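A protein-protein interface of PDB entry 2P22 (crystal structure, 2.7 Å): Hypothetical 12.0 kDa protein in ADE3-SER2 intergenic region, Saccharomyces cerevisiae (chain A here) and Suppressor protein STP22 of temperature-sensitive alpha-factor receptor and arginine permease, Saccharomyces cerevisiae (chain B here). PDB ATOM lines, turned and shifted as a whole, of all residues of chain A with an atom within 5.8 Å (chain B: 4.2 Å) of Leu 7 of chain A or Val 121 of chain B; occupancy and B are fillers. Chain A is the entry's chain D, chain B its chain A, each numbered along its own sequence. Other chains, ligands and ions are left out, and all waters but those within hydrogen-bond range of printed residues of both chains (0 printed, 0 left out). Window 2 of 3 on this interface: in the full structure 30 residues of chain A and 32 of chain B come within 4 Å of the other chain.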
ATOM      1  N   ASN A   2       0.176  -9.074   0.001  1.00  0.00           N
ATOM      2  CA  ASN A   2       1.029  -8.633   1.090  1.00  0.00           C
ATOM      3  C   ASN A   2       2.489  -8.904   0.754  1.00  0.00           C
ATOM      4  O   ASN A   2       3.312  -7.988   0.738  1.00  0.00           O
ATOM      5  CB  ASN A   2       0.643  -9.366   2.376  1.00  0.00           C
ATOM      6  CG  ASN A   2       1.380  -8.843   3.587  1.00  0.00           C
ATOM      7  OD1 ASN A   2       2.575  -9.080   3.747  1.00  0.00           O
ATOM      8  ND2 ASN A   2       0.671  -8.121   4.448  1.00  0.00           N
ATOM      9  N   VAL A   3       2.806 -10.163   0.474  1.00  0.00           N
ATOM     10  CA  VAL A   3       4.174 -10.543   0.142  1.00  0.00           C
ATOM     11  C   VAL A   3       4.539 -10.026  -1.237  1.00  0.00           C
ATOM     12  O   VAL A   3       5.658  -9.558  -1.465  1.00  0.00           O
ATOM     13  CB  VAL A   3       4.346 -12.064   0.141  1.00  0.00           C
ATOM     14  CG1 VAL A   3       5.824 -12.408   0.056  1.00  0.00           C
ATOM     15  CG2 VAL A   3       3.722 -12.653   1.392  1.00  0.00           C
ATOM     16  N   GLU A   4       3.583 -10.135  -2.154  1.00  0.00           N
ATOM     17  CA  GLU A   4       3.749  -9.672  -3.527  1.00  0.00           C
ATOM     18  C   GLU A   4       4.226  -8.220  -3.512  1.00  0.00           C
ATOM     19  O   GLU A   4       5.228  -7.860  -4.135  1.00  0.00           O
ATOM     20  CB  GLU A   4       2.408  -9.743  -4.255  1.00  0.00           C
ATOM     21  CG  GLU A   4       2.404 -10.586  -5.508  1.00  0.00           C
ATOM     22  CD  GLU A   4       2.616 -12.053  -5.217  1.00  0.00           C
ATOM     23  OE1 GLU A   4       1.902 -12.596  -4.345  1.00  0.00           O
ATOM     24  OE2 GLU A   4       3.487 -12.663  -5.872  1.00  0.00           O
ATOM     25  N   GLU A   5       3.483  -7.393  -2.785  1.00  0.00           N
ATOM     26  CA  GLU A   5       3.776  -5.979  -2.660  1.00  0.00           C
ATOM     27  C   GLU A   5       5.158  -5.761  -2.072  1.00  0.00           C
ATOM     28  O   GLU A   5       5.988  -5.076  -2.669  1.00  0.00           O
ATOM     29  CB  GLU A   5       2.724  -5.313  -1.777  1.00  0.00           C
ATOM     30  CG  GLU A   5       2.708  -3.805  -1.894  1.00  0.00           C
ATOM     31  CD  GLU A   5       1.616  -3.158  -1.063  1.00  0.00           C
ATOM     32  OE1 GLU A   5       1.488  -1.912  -1.130  1.00  0.00           O
ATOM     33  OE2 GLU A   5       0.894  -3.894  -0.349  1.00  0.00           O
ATOM     34  N   LEU A   6       5.400  -6.350  -0.903  1.00  0.00           N
ATOM     35  CA  LEU A   6       6.690  -6.232  -0.225  1.00  0.00           C
ATOM     36  C   LEU A   6       7.837  -6.513  -1.190  1.00  0.00           C
ATOM     37  O   LEU A   6       8.773  -5.722  -1.286  1.00  0.00           O
ATOM     38  CB  LEU A   6       6.766  -7.203   0.966  1.00  0.00           C
ATOM     39  CG  LEU A   6       7.924  -7.031   1.973  1.00  0.00           C
ATOM     40  CD1 LEU A   6       7.586  -7.755   3.270  1.00  0.00           C
ATOM     41  CD2 LEU A   6       9.232  -7.551   1.400  1.00  0.00           C
ATOM     42  N   LEU A   7       7.759  -7.634  -1.905  1.00  0.00           N
ATOM     43  CA  LEU A   7       8.799  -8.007  -2.854  1.00  0.00           C
ATOM     44  C   LEU A   7       9.084  -6.924  -3.889  1.00  0.00           C
ATOM     45  O   LEU A   7      10.233  -6.488  -4.034  1.00  0.00           O
ATOM     46  CB  LEU A   7       8.429  -9.311  -3.566  1.00  0.00           C
ATOM     47  CG  LEU A   7       8.521 -10.598  -2.734  1.00  0.00           C
ATOM     48  CD1 LEU A   7       7.849 -11.760  -3.451  1.00  0.00           C
ATOM     49  CD2 LEU A   7       9.989 -10.903  -2.466  1.00  0.00           C
ATOM     50  N   ARG A   8       8.036  -6.495  -4.596  1.00  0.00           N
ATOM     51  CA  ARG A   8       8.152  -5.475  -5.641  1.00  0.00           C
ATOM     52  C   ARG A   8       8.426  -4.102  -5.062  1.00  0.00           C
ATOM     53  O   ARG A   8       8.945  -3.223  -5.743  1.00  0.00           O
ATOM     54  CB  ARG A   8       6.877  -5.417  -6.502  1.00  0.00           C
ATOM     55  CG  ARG A   8       5.620  -4.930  -5.773  1.00  0.00           C
ATOM     56  CD  ARG A   8       4.429  -4.767  -6.734  1.00  0.00           C
ATOM     57  NE  ARG A   8       4.116  -5.998  -7.463  1.00  0.00           N
ATOM     58  CZ  ARG A   8       3.062  -6.777  -7.229  1.00  0.00           C
ATOM     59  NH1 ARG A   8       2.190  -6.467  -6.271  1.00  0.00           N
ATOM     60  NH2 ARG A   8       2.888  -7.874  -7.958  1.00  0.00           N
ATOM     61  N   ARG A   9       8.073  -3.913  -3.803  1.00  0.00           N
ATOM     62  CA  ARG A   9       8.301  -2.631  -3.168  1.00  0.00           C
ATOM     63  C   ARG A   9       9.766  -2.453  -2.832  1.00  0.00           C
ATOM     64  O   ARG A   9      10.199  -1.358  -2.487  1.00  0.00           O
ATOM     65  CB  ARG A   9       7.426  -2.498  -1.919  1.00  0.00           C
ATOM     66  CG  ARG A   9       6.136  -1.682  -2.155  1.00  0.00           C
ATOM     67  CD  ARG A   9       5.416  -2.069  -3.467  1.00  0.00           C
ATOM     68  NE  ARG A   9       4.138  -1.368  -3.655  1.00  0.00           N
ATOM     69  CZ  ARG A   9       3.392  -1.419  -4.761  1.00  0.00           C
ATOM     70  NH1 ARG A   9       3.781  -2.133  -5.807  1.00  0.00           N
ATOM     71  NH2 ARG A   9       2.241  -0.764  -4.818  1.00  0.00           N
ATOM     72  N   ILE A  10      10.531  -3.534  -2.941  1.00  0.00           N
ATOM     73  CA  ILE A  10      11.963  -3.478  -2.662  1.00  0.00           C
ATOM     74  C   ILE A  10      12.719  -3.712  -3.954  1.00  0.00           C
ATOM     75  O   ILE A  10      12.496  -4.707  -4.639  1.00  0.00           O
ATOM     76  CB  ILE A  10      12.398  -4.540  -1.659  1.00  0.00           C
ATOM     77  CG1 ILE A  10      11.656  -4.343  -0.337  1.00  0.00           C
ATOM     78  CG2 ILE A  10      13.907  -4.466  -1.457  1.00  0.00           C
ATOM     79  CD1 ILE A  10      11.889  -5.463   0.663  1.00  0.00           C
ATOM     80  N   PRO A  11      13.650  -2.804  -4.286  1.00  0.00           N
ATOM     81  CA  PRO A  11      14.478  -2.843  -5.498  1.00  0.00           C
ATOM     82  C   PRO A  11      15.471  -3.999  -5.645  1.00  0.00           C
ATOM     83  O   PRO A  11      16.119  -4.418  -4.683  1.00  0.00           O
ATOM     84  CB  PRO A  11      15.175  -1.487  -5.470  1.00  0.00           C
ATOM     85  CG  PRO A  11      15.381  -1.260  -3.998  1.00  0.00           C
ATOM     86  CD  PRO A  11      14.046  -1.676  -3.417  1.00  0.00           C
ATOM     87  N   LEU B 117      12.034 -15.542  -0.261  1.00  0.00           N
ATOM     88  CA  LEU B 117      10.656 -15.130  -0.453  1.00  0.00           C
ATOM     89  C   LEU B 117      10.220 -15.248  -1.922  1.00  0.00           C
ATOM     90  O   LEU B 117       9.164 -15.827  -2.218  1.00  0.00           O
ATOM     91  CB  LEU B 117      10.476 -13.702   0.059  1.00  0.00           C
ATOM     92  CG  LEU B 117       9.498 -13.567   1.231  1.00  0.00           C
ATOM     93  CD1 LEU B 117       9.211 -14.902   1.827  1.00  0.00           C
ATOM     94  CD2 LEU B 117      10.058 -12.618   2.248  1.00  0.00           C
ATOM     95  N   TYR B 118      11.028 -14.707  -2.835  1.00  0.00           N
ATOM     96  CA  TYR B 118      10.727 -14.805  -4.265  1.00  0.00           C
ATOM     97  C   TYR B 118      10.477 -16.280  -4.660  1.00  0.00           C
ATOM     98  O   TYR B 118       9.451 -16.625  -5.257  1.00  0.00           O
ATOM     99  CB  TYR B 118      11.887 -14.247  -5.111  1.00  0.00           C
ATOM    100  CG  TYR B 118      11.881 -12.739  -5.313  1.00  0.00           C
ATOM    101  CD1 TYR B 118      12.616 -11.906  -4.486  1.00  0.00           C
ATOM    102  CD2 TYR B 118      11.132 -12.149  -6.335  1.00  0.00           C
ATOM    103  CE1 TYR B 118      12.610 -10.528  -4.663  1.00  0.00           C
ATOM    104  CE2 TYR B 118      11.112 -10.765  -6.523  1.00  0.00           C
ATOM    105  CZ  TYR B 118      11.857  -9.957  -5.679  1.00  0.00           C
ATOM    106  OH  TYR B 118      11.852  -8.586  -5.822  1.00  0.00           O
ATOM    107  N   ASN B 119      11.420 -17.148  -4.312  1.00  0.00           N
ATOM    108  CA  ASN B 119      11.309 -18.558  -4.636  1.00  0.00           C
ATOM    109  C   ASN B 119      10.099 -19.218  -4.020  1.00  0.00           C
ATOM    110  O   ASN B 119       9.462 -20.054  -4.650  1.00  0.00           O
ATOM    111  CB  ASN B 119      12.569 -19.291  -4.195  1.00  0.00           C
ATOM    112  CG  ASN B 119      13.746 -18.979  -5.072  1.00  0.00           C
ATOM    113  OD1 ASN B 119      14.082 -17.821  -5.283  1.00  0.00           O
ATOM    114  ND2 ASN B 119      14.379 -20.016  -5.601  1.00  0.00           N
ATOM    115  N   LEU B 120       9.778 -18.870  -2.780  1.00  0.00           N
ATOM    116  CA  LEU B 120       8.615 -19.479  -2.153  1.00  0.00           C
ATOM    117  C   LEU B 120       7.359 -19.055  -2.892  1.00  0.00           C
ATOM    118  O   LEU B 120       6.471 -19.876  -3.140  1.00  0.00           O
ATOM    119  CB  LEU B 120       8.509 -19.075  -0.687  1.00  0.00           C
ATOM    120  CG  LEU B 120       9.562 -19.621   0.276  1.00  0.00           C
ATOM    121  CD1 LEU B 120       9.251 -19.032   1.623  1.00  0.00           C
ATOM    122  CD2 LEU B 120       9.565 -21.145   0.335  1.00  0.00           C
ATOM    123  N   VAL B 121       7.291 -17.773  -3.248  1.00  0.00           N
ATOM    124  CA  VAL B 121       6.139 -17.263  -3.980  1.00  0.00           C
ATOM    125  C   VAL B 121       6.028 -17.989  -5.320  1.00  0.00           C
ATOM    126  O   VAL B 121       4.967 -18.517  -5.672  1.00  0.00           O
ATOM    127  CB  VAL B 121       6.262 -15.753  -4.213  1.00  0.00           C
ATOM    128  CG1 VAL B 121       5.034 -15.226  -4.937  1.00  0.00           C
ATOM    129  CG2 VAL B 121       6.425 -15.060  -2.890  1.00  0.00           C
ATOM    130  N   ALA B 122       7.131 -18.022  -6.060  1.00  0.00           N
ATOM    131  CA  ALA B 122       7.154 -18.718  -7.334  1.00  0.00           C
ATOM    132  C   ALA B 122       6.681 -20.162  -7.131  1.00  0.00           C
ATOM    133  O   ALA B 122       5.768 -20.624  -7.805  1.00  0.00           O
ATOM    134  CB  ALA B 122       8.554 -18.689  -7.920  1.00  0.00           C
ATOM    135  N   GLN B 123       7.284 -20.873  -6.192  1.00  0.00           N
ATOM    136  CA  GLN B 123       6.874 -22.251  -5.930  1.00  0.00           C
ATOM    137  C   GLN B 123       5.387 -22.391  -5.646  1.00  0.00           C
ATOM    138  O   GLN B 123       4.782 -23.406  -5.986  1.00  0.00           O
ATOM    139  CB  GLN B 123       7.625 -22.814  -4.730  1.00  0.00           C
ATOM    140  CG  GLN B 123       9.107 -22.832  -4.905  1.00  0.00           C
ATOM    141  CD  GLN B 123       9.800 -23.439  -3.722  1.00  0.00           C
ATOM    142  OE1 GLN B 123       9.421 -24.524  -3.258  1.00  0.00           O
ATOM    143  NE2 GLN B 123      10.833 -22.756  -3.227  1.00  0.00           N
ATOM    144  N   ASP B 124       4.811 -21.384  -4.993  1.00  0.00           N
ATOM    145  CA  ASP B 124       3.393 -21.392  -4.628  1.00  0.00           C
ATOM    146  C   ASP B 124       2.525 -21.414  -5.865  1.00  0.00           C
ATOM    147  O   ASP B 124       1.631 -22.253  -5.982  1.00  0.00           O
ATOM    148  CB  ASP B 124       3.068 -20.155  -3.791  1.00  0.00           C
ATOM    149  CG  ASP B 124       1.632 -20.127  -3.311  1.00  0.00           C
ATOM    150  OD1 ASP B 124       1.027 -21.209  -3.155  1.00  0.00           O
ATOM    151  OD2 ASP B 124       1.105 -19.020  -3.065  1.00  0.00           O
ATOM    152  N   TYR B 125       2.795 -20.481  -6.779  1.00  0.00           N
ATOM    153  CA  TYR B 125       2.056 -20.387  -8.028  1.00  0.00           C
ATOM    154  C   TYR B 125       2.299 -21.632  -8.855  1.00  0.00           C
ATOM    155  O   TYR B 125       1.356 -22.334  -9.252  1.00  0.00           O
ATOM    156  CB  TYR B 125       2.499 -19.166  -8.828  1.00  0.00           C
ATOM    157  CG  TYR B 125       1.865 -17.890  -8.358  1.00  0.00           C
ATOM    158  CD1 TYR B 125       2.284 -17.276  -7.182  1.00  0.00           C
ATOM    159  CD2 TYR B 125       0.823 -17.299  -9.080  1.00  0.00           C
ATOM    160  CE1 TYR B 125       1.688 -16.106  -6.733  1.00  0.00           C
ATOM    161  CE2 TYR B 125       0.215 -16.124  -8.635  1.00  0.00           C
ATOM    162  CZ  TYR B 125       0.660 -15.536  -7.460  1.00  0.00           C
ATOM    163  OH  TYR B 125       0.108 -14.368  -7.004  1.00  0.00           O
ATOM    164  N   ILE B 166       5.859 -19.072   4.037  1.00  0.00           N
ATOM    165  CA  ILE B 166       5.883 -17.672   3.656  1.00  0.00           C
ATOM    166  C   ILE B 166       5.262 -16.891   4.786  1.00  0.00           C
ATOM    167  O   ILE B 166       5.780 -15.865   5.209  1.00  0.00           O
ATOM    168  CB  ILE B 166       5.091 -17.449   2.350  1.00  0.00           C
ATOM    169  CG1 ILE B 166       5.844 -18.116   1.196  1.00  0.00           C
ATOM    170  CG2 ILE B 166       4.916 -15.968   2.071  1.00  0.00           C
ATOM    171  CD1 ILE B 166       5.183 -17.996  -0.146  1.00  0.00           C
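The backbone carbonyl oxygen (O) of Leu 7 of chain A lies within hydrogen-bond range of the side-chain hydroxyl (OH) of Tyr 118 of chain B.
Among the printed residues, merely in contact across the chains: Val 3 of chain A with Ile 166 of chain B, Glu 4 of chain A with Val 121 of chain B, Glu 4 of chain A with Tyr 125 of chain B, Leu 7 of chain A with Leu 117 of chain B and Leu 7 of chain A with Val 121 of chain B.
Of the printed residues of chain A, Val 121 of chain B touches Glu 4 (3.1 Å) and Leu 7 (3.6 Å). Of the printed residues of chain B, Glu 4 of chain A touches Val 121 and Tyr 125. Of the printed residues of chain A, Tyr 118 of chain B touches Leu 7 (3.2 Å). Of the printed residues of chain A, Ile 166 of chain B touches Val 3 (3.6 Å). The nearest printed residue of chain B that does not touch Leu 7 of chain A is Asn 119 of chain B (6.5 Å). The nearest printed residue of chain A that does not touch Ile 166 of chain B is Glu 4 of chain A (7.3 Å).
Of the 10 printed residues of chain A, 3 touch a printed residue of chain B. Hydrophobic or aromatic side chains of chain A within 4 Å of the printed part of chain B: Val 3 and Leu 7. Hydrophobic or aromatic side chains of chain B that line the printed part of chain A: Leu 117, Tyr 118, Val 121, Tyr 125 and Ile 166.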
